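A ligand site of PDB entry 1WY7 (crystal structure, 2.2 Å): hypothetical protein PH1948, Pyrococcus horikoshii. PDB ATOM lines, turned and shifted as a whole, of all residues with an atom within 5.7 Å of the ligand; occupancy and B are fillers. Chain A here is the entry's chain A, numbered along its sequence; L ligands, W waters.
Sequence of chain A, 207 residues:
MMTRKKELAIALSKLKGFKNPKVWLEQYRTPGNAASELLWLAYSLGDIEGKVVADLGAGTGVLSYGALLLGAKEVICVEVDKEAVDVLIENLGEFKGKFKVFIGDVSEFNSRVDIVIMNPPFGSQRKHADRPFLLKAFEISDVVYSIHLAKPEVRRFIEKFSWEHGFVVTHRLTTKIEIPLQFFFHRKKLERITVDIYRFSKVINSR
A nitrogen (N5) of the ligand is in hydrogen-bond range of the backbone NH (N) of Val 106.
A nitrogen (N6) of the ligand lies within hydrogen-bond range of the backbone NH (N) of Val 80 (3.4 Å).
OD2 of Asp 105 sits at hydrogen-bond distance from N4 of the ligand (2.7 Å).
The side-chain carboxylate of Glu 79 is in hydrogen-bond range of an oxygen (O5) of the ligand (2.6 Å).
O2 of the ligand lies within hydrogen-bond range of OG1 of Thr 30 (2.9 Å).
N of Val 62 lies within hydrogen-bond range of O1 of the ligand (2.8 Å).
OG1 of Thr 60 sits at hydrogen-bond distance from N1 of the ligand, 3.3 Å away.
O5 of the ligand sits at hydrogen-bond distance from NE2 of Gln 27 (2.8 Å).
N of Thr 60 sits close to N1 of the ligand (3.5 Å).
S1 of the ligand sits close to O of Glu 26, 3.2 Å away.
An oxygen (O1) of the ligand lies close to the backbone carbonyl oxygen (O) of Ala 58 (3.5 Å).
A sulfur (S1) of the ligand lies close to the backbone carbonyl oxygen (O) of Asn 119 (3.7 Å).
CZ of Phe 18 touches O4 of the ligand (3.2 Å).
Leu 25 touches the ligand (O to C8, 3.6 Å).
O of Tyr 28 touches C3 of the ligand, at 2.8 Å.
CA of Arg 29 touches N1 of the ligand (3.1 Å).
O of Gly 57 touches C5 of the ligand, at 3.2 Å.
Gly 59 touches the ligand.
Gly 61 touches the ligand (N to O1, 3.6 Å).
Leu 63 touches the ligand (CG to O2, 3.9 Å).
Gly 104 touches the ligand.
Phe 133 touches the ligand (CZ to C14, 3.4 Å).
Hydrophobic or aromatic side chains that line the ligand: Phe 18, Leu 25, Val 62, Leu 63, Val 80, Val 106 and Phe 133.
Water W2 lies within hydrogen-bond range of an oxygen (O2) of the ligand, the side-chain carboxylate (OD1) of Asp 55, the backbone carbonyl oxygen (O) of Ala 58, the backbone NH (N) of Leu 63 and the backbone NH (N) of Val 62.
OE1 of Glu 79 lies within hydrogen-bond range of N of Gly 59, 2.8 Å away.
The side-chain carboxylate of Asp 105 sits at hydrogen-bond distance from the side-chain hydroxyl of Ser 107.
The backbone carbonyl oxygen (O) of Val 78 sits at hydrogen-bond distance from the backbone NH (N) of Gly 57.
OH of Tyr 28 lies within hydrogen-bond range of ND2 of Asn 119 (3.1 Å).
O of Glu 79 sits at hydrogen-bond distance from N of Gly 104, at 3.2 Å.
O of Val 78 is in hydrogen-bond range of N of Ala 58, at 2.9 Å.
The side-chain amide oxygen (OD1) of Asn 119 lies within hydrogen-bond range of the side-chain hydroxyl (OG1) of Thr 30 (2.7 Å).
The side-chain carboxylate of Glu 79 is in hydrogen-bond range of the backbone NH of Asp 81.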
ATOM      1  N   PHE A  18     -29.498 -30.186 -25.760  1.00  0.00           N
ATOM      2  CA  PHE A  18     -28.942 -30.674 -24.488  1.00  0.00           C
ATOM      3  C   PHE A  18     -29.983 -31.372 -23.619  1.00  0.00           C
ATOM      4  O   PHE A  18     -31.102 -30.891 -23.480  1.00  0.00           O
ATOM      5  CB  PHE A  18     -28.347 -29.523 -23.684  1.00  0.00           C
ATOM      6  CG  PHE A  18     -27.103 -28.925 -24.263  1.00  0.00           C
ATOM      7  CD1 PHE A  18     -27.171 -27.858 -25.145  1.00  0.00           C
ATOM      8  CD2 PHE A  18     -25.852 -29.429 -23.905  1.00  0.00           C
ATOM      9  CE1 PHE A  18     -26.013 -27.286 -25.670  1.00  0.00           C
ATOM     10  CE2 PHE A  18     -24.680 -28.858 -24.420  1.00  0.00           C
ATOM     11  CZ  PHE A  18     -24.760 -27.786 -25.303  1.00  0.00           C
ATOM     12  N   LEU A  25     -22.109 -23.414 -17.653  1.00  0.00           N
ATOM     13  CA  LEU A  25     -21.228 -23.754 -18.752  1.00  0.00           C
ATOM     14  C   LEU A  25     -21.806 -23.168 -20.047  1.00  0.00           C
ATOM     15  O   LEU A  25     -21.319 -23.470 -21.146  1.00  0.00           O
ATOM     16  CB  LEU A  25     -21.107 -25.280 -18.911  1.00  0.00           C
ATOM     17  CG  LEU A  25     -20.392 -26.103 -17.847  1.00  0.00           C
ATOM     18  CD1 LEU A  25     -20.311 -27.561 -18.318  1.00  0.00           C
ATOM     19  CD2 LEU A  25     -18.994 -25.550 -17.622  1.00  0.00           C
ATOM     20  N   GLU A  26     -22.836 -22.342 -19.901  1.00  0.00           N
ATOM     21  CA  GLU A  26     -23.505 -21.712 -21.027  1.00  0.00           C
ATOM     22  C   GLU A  26     -23.895 -22.731 -22.094  1.00  0.00           C
ATOM     23  O   GLU A  26     -23.542 -22.576 -23.262  1.00  0.00           O
ATOM     24  CB  GLU A  26     -22.596 -20.651 -21.670  1.00  0.00           C
ATOM     25  CG  GLU A  26     -22.227 -19.475 -20.767  1.00  0.00           C
ATOM     26  CD  GLU A  26     -21.716 -18.285 -21.564  1.00  0.00           C
ATOM     27  OE1 GLU A  26     -21.120 -17.369 -20.961  1.00  0.00           O
ATOM     28  OE2 GLU A  26     -21.917 -18.269 -22.793  1.00  0.00           O
ATOM     29  N   GLN A  27     -24.618 -23.766 -21.694  1.00  0.00           N
ATOM     30  CA  GLN A  27     -25.023 -24.801 -22.645  1.00  0.00           C
ATOM     31  C   GLN A  27     -26.359 -24.557 -23.334  1.00  0.00           C
ATOM     32  O   GLN A  27     -27.425 -24.834 -22.784  1.00  0.00           O
ATOM     33  CB  GLN A  27     -25.054 -26.181 -21.985  1.00  0.00           C
ATOM     34  CG  GLN A  27     -23.695 -26.680 -21.483  1.00  0.00           C
ATOM     35  CD  GLN A  27     -23.735 -28.125 -20.980  1.00  0.00           C
ATOM     36  OE1 GLN A  27     -24.757 -28.582 -20.444  1.00  0.00           O
ATOM     37  NE2 GLN A  27     -22.641 -28.845 -21.144  1.00  0.00           N
ATOM     38  N   TYR A  28     -26.294 -24.012 -24.544  1.00  0.00           N
ATOM     39  CA  TYR A  28     -27.462 -23.786 -25.370  1.00  0.00           C
ATOM     40  C   TYR A  28     -26.978 -24.138 -26.774  1.00  0.00           C
ATOM     41  O   TYR A  28     -25.874 -23.781 -27.165  1.00  0.00           O
ATOM     42  CB  TYR A  28     -27.949 -22.326 -25.295  1.00  0.00           C
ATOM     43  CG  TYR A  28     -26.979 -21.298 -25.847  1.00  0.00           C
ATOM     44  CD1 TYR A  28     -26.879 -21.077 -27.220  1.00  0.00           C
ATOM     45  CD2 TYR A  28     -26.130 -20.587 -24.998  1.00  0.00           C
ATOM     46  CE1 TYR A  28     -25.934 -20.192 -27.746  1.00  0.00           C
ATOM     47  CE2 TYR A  28     -25.183 -19.699 -25.515  1.00  0.00           C
ATOM     48  CZ  TYR A  28     -25.096 -19.509 -26.896  1.00  0.00           C
ATOM     49  OH  TYR A  28     -24.119 -18.697 -27.410  1.00  0.00           O
ATOM     50  N   ARG A  29     -27.776 -24.875 -27.523  1.00  0.00           N
ATOM     51  CA  ARG A  29     -27.397 -25.262 -28.876  1.00  0.00           C
ATOM     52  C   ARG A  29     -27.243 -24.016 -29.751  1.00  0.00           C
ATOM     53  O   ARG A  29     -28.011 -23.062 -29.605  1.00  0.00           O
ATOM     54  CB  ARG A  29     -28.462 -26.174 -29.477  1.00  0.00           C
ATOM     55  CG  ARG A  29     -29.829 -25.513 -29.522  1.00  0.00           C
ATOM     56  CD  ARG A  29     -30.839 -26.383 -30.223  1.00  0.00           C
ATOM     57  NE  ARG A  29     -30.356 -26.776 -31.535  1.00  0.00           N
ATOM     58  CZ  ARG A  29     -31.029 -27.580 -32.363  1.00  0.00           C
ATOM     59  NH1 ARG A  29     -30.506 -27.889 -33.540  1.00  0.00           N
ATOM     60  NH2 ARG A  29     -32.213 -28.048 -32.015  1.00  0.00           N
ATOM     61  N   THR A  30     -26.270 -24.020 -30.656  1.00  0.00           N
ATOM     62  CA  THR A  30     -26.091 -22.866 -31.531  1.00  0.00           C
ATOM     63  C   THR A  30     -27.325 -22.751 -32.424  1.00  0.00           C
ATOM     64  O   THR A  30     -27.648 -23.689 -33.154  1.00  0.00           O
ATOM     65  CB  THR A  30     -24.855 -23.014 -32.451  1.00  0.00           C
ATOM     66  OG1 THR A  30     -23.683 -23.287 -31.673  1.00  0.00           O
ATOM     67  CG2 THR A  30     -24.637 -21.720 -33.235  1.00  0.00           C
ATOM     68  N   ASP A  55     -14.004 -28.173 -33.555  1.00  0.00           N
ATOM     69  CA  ASP A  55     -15.198 -27.491 -33.061  1.00  0.00           C
ATOM     70  C   ASP A  55     -15.003 -27.383 -31.532  1.00  0.00           C
ATOM     71  O   ASP A  55     -15.231 -28.353 -30.806  1.00  0.00           O
ATOM     72  CB  ASP A  55     -16.435 -28.338 -33.403  1.00  0.00           C
ATOM     73  CG  ASP A  55     -17.727 -27.695 -32.955  1.00  0.00           C
ATOM     74  OD1 ASP A  55     -18.809 -28.296 -33.196  1.00  0.00           O
ATOM     75  OD2 ASP A  55     -17.684 -26.580 -32.371  1.00  0.00           O
ATOM     76  N   LEU A  56     -14.559 -26.215 -31.069  1.00  0.00           N
ATOM     77  CA  LEU A  56     -14.314 -25.999 -29.643  1.00  0.00           C
ATOM     78  C   LEU A  56     -15.616 -25.689 -28.915  1.00  0.00           C
ATOM     79  O   LEU A  56     -16.343 -24.753 -29.297  1.00  0.00           O
ATOM     80  CB  LEU A  56     -13.271 -24.891 -29.458  1.00  0.00           C
ATOM     81  CG  LEU A  56     -11.794 -25.308 -29.544  1.00  0.00           C
ATOM     82  CD1 LEU A  56     -11.584 -26.421 -30.554  1.00  0.00           C
ATOM     83  CD2 LEU A  56     -10.935 -24.098 -29.890  1.00  0.00           C
ATOM     84  N   GLY A  57     -15.892 -26.467 -27.866  1.00  0.00           N
ATOM     85  CA  GLY A  57     -17.135 -26.319 -27.118  1.00  0.00           C
ATOM     86  C   GLY A  57     -18.231 -26.865 -28.016  1.00  0.00           C
ATOM     87  O   GLY A  57     -19.298 -26.254 -28.171  1.00  0.00           O
ATOM     88  N   ALA A  58     -17.967 -28.028 -28.604  1.00  0.00           N
ATOM     89  CA  ALA A  58     -18.891 -28.680 -29.551  1.00  0.00           C
ATOM     90  C   ALA A  58     -20.323 -28.905 -29.076  1.00  0.00           C
ATOM     91  O   ALA A  58     -21.256 -28.952 -29.886  1.00  0.00           O
ATOM     92  CB  ALA A  58     -18.288 -30.005 -30.040  1.00  0.00           C
ATOM     93  N   GLY A  59     -20.506 -29.048 -27.765  1.00  0.00           N
ATOM     94  CA  GLY A  59     -21.837 -29.247 -27.217  1.00  0.00           C
ATOM     95  C   GLY A  59     -22.626 -30.367 -27.876  1.00  0.00           C
ATOM     96  O   GLY A  59     -22.200 -31.537 -27.848  1.00  0.00           O
ATOM     97  N   THR A  60     -23.771 -30.023 -28.469  1.00  0.00           N
ATOM     98  CA  THR A  60     -24.616 -31.014 -29.147  1.00  0.00           C
ATOM     99  C   THR A  60     -24.144 -31.318 -30.567  1.00  0.00           C
ATOM    100  O   THR A  60     -24.681 -32.220 -31.215  1.00  0.00           O
ATOM    101  CB  THR A  60     -26.098 -30.592 -29.224  1.00  0.00           C
ATOM    102  OG1 THR A  60     -26.231 -29.379 -29.980  1.00  0.00           O
ATOM    103  CG2 THR A  60     -26.664 -30.393 -27.848  1.00  0.00           C
ATOM    104  N   GLY A  61     -23.154 -30.571 -31.048  1.00  0.00           N
ATOM    105  CA  GLY A  61     -22.631 -30.802 -32.385  1.00  0.00           C
ATOM    106  C   GLY A  61     -23.263 -30.079 -33.563  1.00  0.00           C
ATOM    107  O   GLY A  61     -23.067 -30.487 -34.698  1.00  0.00           O
ATOM    108  N   VAL A  62     -23.983 -28.981 -33.327  1.00  0.00           N
ATOM    109  CA  VAL A  62     -24.598 -28.254 -34.444  1.00  0.00           C
ATOM    110  C   VAL A  62     -23.570 -27.785 -35.472  1.00  0.00           C
ATOM    111  O   VAL A  62     -23.718 -28.045 -36.669  1.00  0.00           O
ATOM    112  CB  VAL A  62     -25.392 -27.012 -33.961  1.00  0.00           C
ATOM    113  CG1 VAL A  62     -25.852 -26.198 -35.155  1.00  0.00           C
ATOM    114  CG2 VAL A  62     -26.584 -27.434 -33.122  1.00  0.00           C
ATOM    115  N   LEU A  63     -22.523 -27.098 -35.009  1.00  0.00           N
ATOM    116  CA  LEU A  63     -21.486 -26.604 -35.897  1.00  0.00           C
ATOM    117  C   LEU A  63     -20.730 -27.752 -36.572  1.00  0.00           C
ATOM    118  O   LEU A  63     -20.397 -27.668 -37.753  1.00  0.00           O
ATOM    119  CB  LEU A  63     -20.499 -25.715 -35.136  1.00  0.00           C
ATOM    120  CG  LEU A  63     -21.051 -24.395 -34.598  1.00  0.00           C
ATOM    121  CD1 LEU A  63     -19.920 -23.587 -33.989  1.00  0.00           C
ATOM    122  CD2 LEU A  63     -21.722 -23.597 -35.734  1.00  0.00           C
ATOM    123  N   VAL A  78     -14.409 -30.848 -29.423  1.00  0.00           N
ATOM    124  CA  VAL A  78     -13.841 -30.623 -28.100  1.00  0.00           C
ATOM    125  C   VAL A  78     -14.967 -30.172 -27.193  1.00  0.00           C
ATOM    126  O   VAL A  78     -15.569 -29.126 -27.418  1.00  0.00           O
ATOM    127  CB  VAL A  78     -12.758 -29.534 -28.109  1.00  0.00           C
ATOM    128  CG1 VAL A  78     -12.223 -29.331 -26.698  1.00  0.00           C
ATOM    129  CG2 VAL A  78     -11.622 -29.918 -29.044  1.00  0.00           C
ATOM    130  N   GLU A  79     -15.242 -30.966 -26.160  1.00  0.00           N
ATOM    131  CA  GLU A  79     -16.314 -30.689 -25.226  1.00  0.00           C
ATOM    132  C   GLU A  79     -15.967 -31.245 -23.844  1.00  0.00           C
ATOM    133  O   GLU A  79     -15.553 -32.402 -23.722  1.00  0.00           O
ATOM    134  CB  GLU A  79     -17.603 -31.317 -25.752  1.00  0.00           C
ATOM    135  CG  GLU A  79     -18.743 -31.369 -24.770  1.00  0.00           C
ATOM    136  CD  GLU A  79     -19.164 -30.007 -24.299  1.00  0.00           C
ATOM    137  OE1 GLU A  79     -19.417 -29.125 -25.150  1.00  0.00           O
ATOM    138  OE2 GLU A  79     -19.238 -29.813 -23.078  1.00  0.00           O
ATOM    139  N   VAL A  80     -16.154 -30.443 -22.795  1.00  0.00           N
ATOM    140  CA  VAL A  80     -15.822 -30.862 -21.431  1.00  0.00           C
ATOM    141  C   VAL A  80     -16.890 -31.731 -20.773  1.00  0.00           C
ATOM    142  O   VAL A  80     -16.597 -32.489 -19.846  1.00  0.00           O
ATOM    143  CB  VAL A  80     -15.586 -29.639 -20.505  1.00  0.00           C
ATOM    144  CG1 VAL A  80     -16.897 -28.910 -20.270  1.00  0.00           C
ATOM    145  CG2 VAL A  80     -14.972 -30.094 -19.178  1.00  0.00           C
ATOM    146  N   ASP A  81     -18.130 -31.627 -21.250  1.00  0.00           N
ATOM    147  CA  ASP A  81     -19.223 -32.365 -20.650  1.00  0.00           C
ATOM    148  C   ASP A  81     -19.665 -33.647 -21.373  1.00  0.00           C
ATOM    149  O   ASP A  81     -20.240 -33.596 -22.465  1.00  0.00           O
ATOM    150  CB  ASP A  81     -20.412 -31.421 -20.472  1.00  0.00           C
ATOM    151  CG  ASP A  81     -21.565 -32.075 -19.734  1.00  0.00           C
ATOM    152  OD1 ASP A  81     -22.621 -31.414 -19.596  1.00  0.00           O
ATOM    153  OD2 ASP A  81     -21.433 -33.235 -19.289  1.00  0.00           O
ATOM    154  N   ALA A  84     -23.091 -33.989 -22.834  1.00  0.00           N
ATOM    155  CA  ALA A  84     -23.316 -33.273 -24.079  1.00  0.00           C
ATOM    156  C   ALA A  84     -22.808 -34.165 -25.216  1.00  0.00           C
ATOM    157  O   ALA A  84     -23.414 -34.216 -26.286  1.00  0.00           O
ATOM    158  CB  ALA A  84     -22.564 -31.942 -24.057  1.00  0.00           C
ATOM    159  N   GLY A 104     -12.708 -33.012 -22.408  1.00  0.00           N
ATOM    160  CA  GLY A 104     -11.800 -32.421 -21.446  1.00  0.00           C
ATOM    161  C   GLY A 104     -11.885 -30.922 -21.616  1.00  0.00           C
ATOM    162  O   GLY A 104     -12.620 -30.461 -22.475  1.00  0.00           O
ATOM    163  N   ASP A 105     -11.142 -30.172 -20.810  1.00  0.00           N
ATOM    164  CA  ASP A 105     -11.175 -28.717 -20.906  1.00  0.00           C
ATOM    165  C   ASP A 105     -10.528 -28.315 -22.221  1.00  0.00           C
ATOM    166  O   ASP A 105      -9.586 -28.962 -22.693  1.00  0.00           O
ATOM    167  CB  ASP A 105     -10.419 -28.085 -19.722  1.00  0.00           C
ATOM    168  CG  ASP A 105     -10.606 -26.573 -19.656  1.00  0.00           C
ATOM    169  OD1 ASP A 105      -9.767 -25.824 -20.191  1.00  0.00           O
ATOM    170  OD2 ASP A 105     -11.621 -26.132 -19.063  1.00  0.00           O
ATOM    171  N   VAL A 106     -11.044 -27.249 -22.812  1.00  0.00           N
ATOM    172  CA  VAL A 106     -10.532 -26.764 -24.096  1.00  0.00           C
ATOM    173  C   VAL A 106      -9.017 -26.494 -24.038  1.00  0.00           C
ATOM    174  O   VAL A 106      -8.306 -26.726 -25.002  1.00  0.00           O
ATOM    175  CB  VAL A 106     -11.284 -25.463 -24.527  1.00  0.00           C
ATOM    176  CG1 VAL A 106     -10.997 -24.321 -23.535  1.00  0.00           C
ATOM    177  CG2 VAL A 106     -10.866 -25.066 -25.947  1.00  0.00           C
ATOM    178  N   SER A 107      -8.521 -26.025 -22.896  1.00  0.00           N
ATOM    179  CA  SER A 107      -7.100 -25.726 -22.782  1.00  0.00           C
ATOM    180  C   SER A 107      -6.205 -26.957 -22.830  1.00  0.00           C
ATOM    181  O   SER A 107      -5.028 -26.820 -23.116  1.00  0.00           O
ATOM    182  CB  SER A 107      -6.804 -24.949 -21.490  1.00  0.00           C
ATOM    183  OG  SER A 107      -7.057 -25.742 -20.342  1.00  0.00           O
ATOM    184  N   ASN A 119     -18.654 -21.699 -30.938  1.00  0.00           N
ATOM    185  CA  ASN A 119     -19.708 -20.890 -30.328  1.00  0.00           C
ATOM    186  C   ASN A 119     -19.322 -21.052 -28.854  1.00  0.00           C
ATOM    187  O   ASN A 119     -19.988 -21.780 -28.114  1.00  0.00           O
ATOM    188  CB  ASN A 119     -21.091 -21.504 -30.587  1.00  0.00           C
ATOM    189  CG  ASN A 119     -22.230 -20.719 -29.956  1.00  0.00           C
ATOM    190  OD1 ASN A 119     -23.376 -21.132 -30.012  1.00  0.00           O
ATOM    191  ND2 ASN A 119     -21.903 -19.577 -29.358  1.00  0.00           N
ATOM    192  N   PRO A 120     -18.225 -20.408 -28.425  1.00  0.00           N
ATOM    193  CA  PRO A 120     -17.746 -20.507 -27.042  1.00  0.00           C
ATOM    194  C   PRO A 120     -18.601 -19.749 -26.052  1.00  0.00           C
ATOM    195  O   PRO A 120     -19.417 -18.925 -26.433  1.00  0.00           O
ATOM    196  CB  PRO A 120     -16.326 -19.939 -27.138  1.00  0.00           C
ATOM    197  CG  PRO A 120     -16.504 -18.825 -28.141  1.00  0.00           C
ATOM    198  CD  PRO A 120     -17.404 -19.456 -29.208  1.00  0.00           C
ATOM    199  N   PRO A 121     -18.439 -20.041 -24.755  1.00  0.00           N
ATOM    200  CA  PRO A 121     -19.238 -19.312 -23.763  1.00  0.00           C
ATOM    201  C   PRO A 121     -18.823 -17.855 -23.848  1.00  0.00           C
ATOM    202  O   PRO A 121     -17.661 -17.560 -24.085  1.00  0.00           O
ATOM    203  CB  PRO A 121     -18.832 -19.972 -22.436  1.00  0.00           C
ATOM    204  CG  PRO A 121     -17.487 -20.534 -22.707  1.00  0.00           C
ATOM    205  CD  PRO A 121     -17.617 -21.080 -24.111  1.00  0.00           C
ATOM    206  N   PHE A 133     -10.771 -20.336 -24.847  1.00  0.00           N
ATOM    207  CA  PHE A 133     -11.148 -20.776 -26.191  1.00  0.00           C
ATOM    208  C   PHE A 133     -10.406 -20.011 -27.302  1.00  0.00           C
ATOM    209  O   PHE A 133      -9.898 -20.609 -28.237  1.00  0.00           O
ATOM    210  CB  PHE A 133     -12.671 -20.657 -26.396  1.00  0.00           C
ATOM    211  CG  PHE A 133     -13.469 -21.687 -25.641  1.00  0.00           C
ATOM    212  CD1 PHE A 133     -13.724 -21.548 -24.275  1.00  0.00           C
ATOM    213  CD2 PHE A 133     -13.938 -22.823 -26.296  1.00  0.00           C
ATOM    214  CE1 PHE A 133     -14.445 -22.536 -23.579  1.00  0.00           C
ATOM    215  CE2 PHE A 133     -14.651 -23.811 -25.612  1.00  0.00           C
ATOM    216  CZ  PHE A 133     -14.907 -23.676 -24.256  1.00  0.00           C
HETATM  217  N1  LIG L   1     -24.593 -26.693 -28.842  1.00  0.00           N
HETATM  218  C1  LIG L   1     -23.653 -25.666 -29.346  1.00  0.00           C
HETATM  219  C2  LIG L   1     -22.594 -25.447 -28.254  1.00  0.00           C
HETATM  220  C3  LIG L   1     -23.111 -24.364 -27.383  1.00  0.00           C
HETATM  221  S1  LIG L   1     -22.269 -23.762 -25.908  1.00  0.00           S
HETATM  222  C4  LIG L   1     -23.134 -26.160 -30.669  1.00  0.00           C
HETATM  223  O1  LIG L   1     -23.814 -27.040 -31.283  1.00  0.00           O
HETATM  224  O2  LIG L   1     -22.032 -25.632 -31.028  1.00  0.00           O
HETATM  225  C5  LIG L   1     -20.583 -24.325 -26.011  1.00  0.00           C
HETATM  226  C6  LIG L   1     -20.131 -25.534 -25.184  1.00  0.00           C
HETATM  227  O3  LIG L   1     -18.926 -25.196 -24.460  1.00  0.00           O
HETATM  228  C7  LIG L   1     -21.060 -25.979 -24.050  1.00  0.00           C
HETATM  229  O4  LIG L   1     -21.710 -27.152 -24.578  1.00  0.00           O
HETATM  230  C8  LIG L   1     -20.156 -26.375 -22.874  1.00  0.00           C
HETATM  231  O5  LIG L   1     -20.341 -27.585 -22.170  1.00  0.00           O
HETATM  232  C9  LIG L   1     -18.749 -26.174 -23.465  1.00  0.00           C
HETATM  233  N2  LIG L   1     -17.751 -25.705 -22.513  1.00  0.00           N
HETATM  234  C10 LIG L   1     -17.860 -24.781 -21.489  1.00  0.00           C
HETATM  235  N3  LIG L   1     -16.741 -24.589 -20.837  1.00  0.00           N
HETATM  236  C11 LIG L   1     -15.832 -25.439 -21.465  1.00  0.00           C
HETATM  237  C12 LIG L   1     -14.450 -25.708 -21.258  1.00  0.00           C
HETATM  238  N4  LIG L   1     -13.731 -25.094 -20.300  1.00  0.00           N
HETATM  239  N5  LIG L   1     -13.811 -26.630 -22.068  1.00  0.00           N
HETATM  240  C13 LIG L   1     -14.531 -27.244 -23.026  1.00  0.00           C
HETATM  241  N6  LIG L   1     -15.844 -27.074 -23.323  1.00  0.00           N
HETATM  242  C14 LIG L   1     -16.448 -26.139 -22.492  1.00  0.00           C
HETATM  243  O   HOH W   1     -16.435 -22.339 -19.353  1.00  0.00           O
HETATM  244  O   HOH W   2     -21.159 -27.676 -32.318  1.00  0.00           O
HETATM  245  O   HOH W   3     -19.112 -24.669 -30.454  1.00  0.00           O
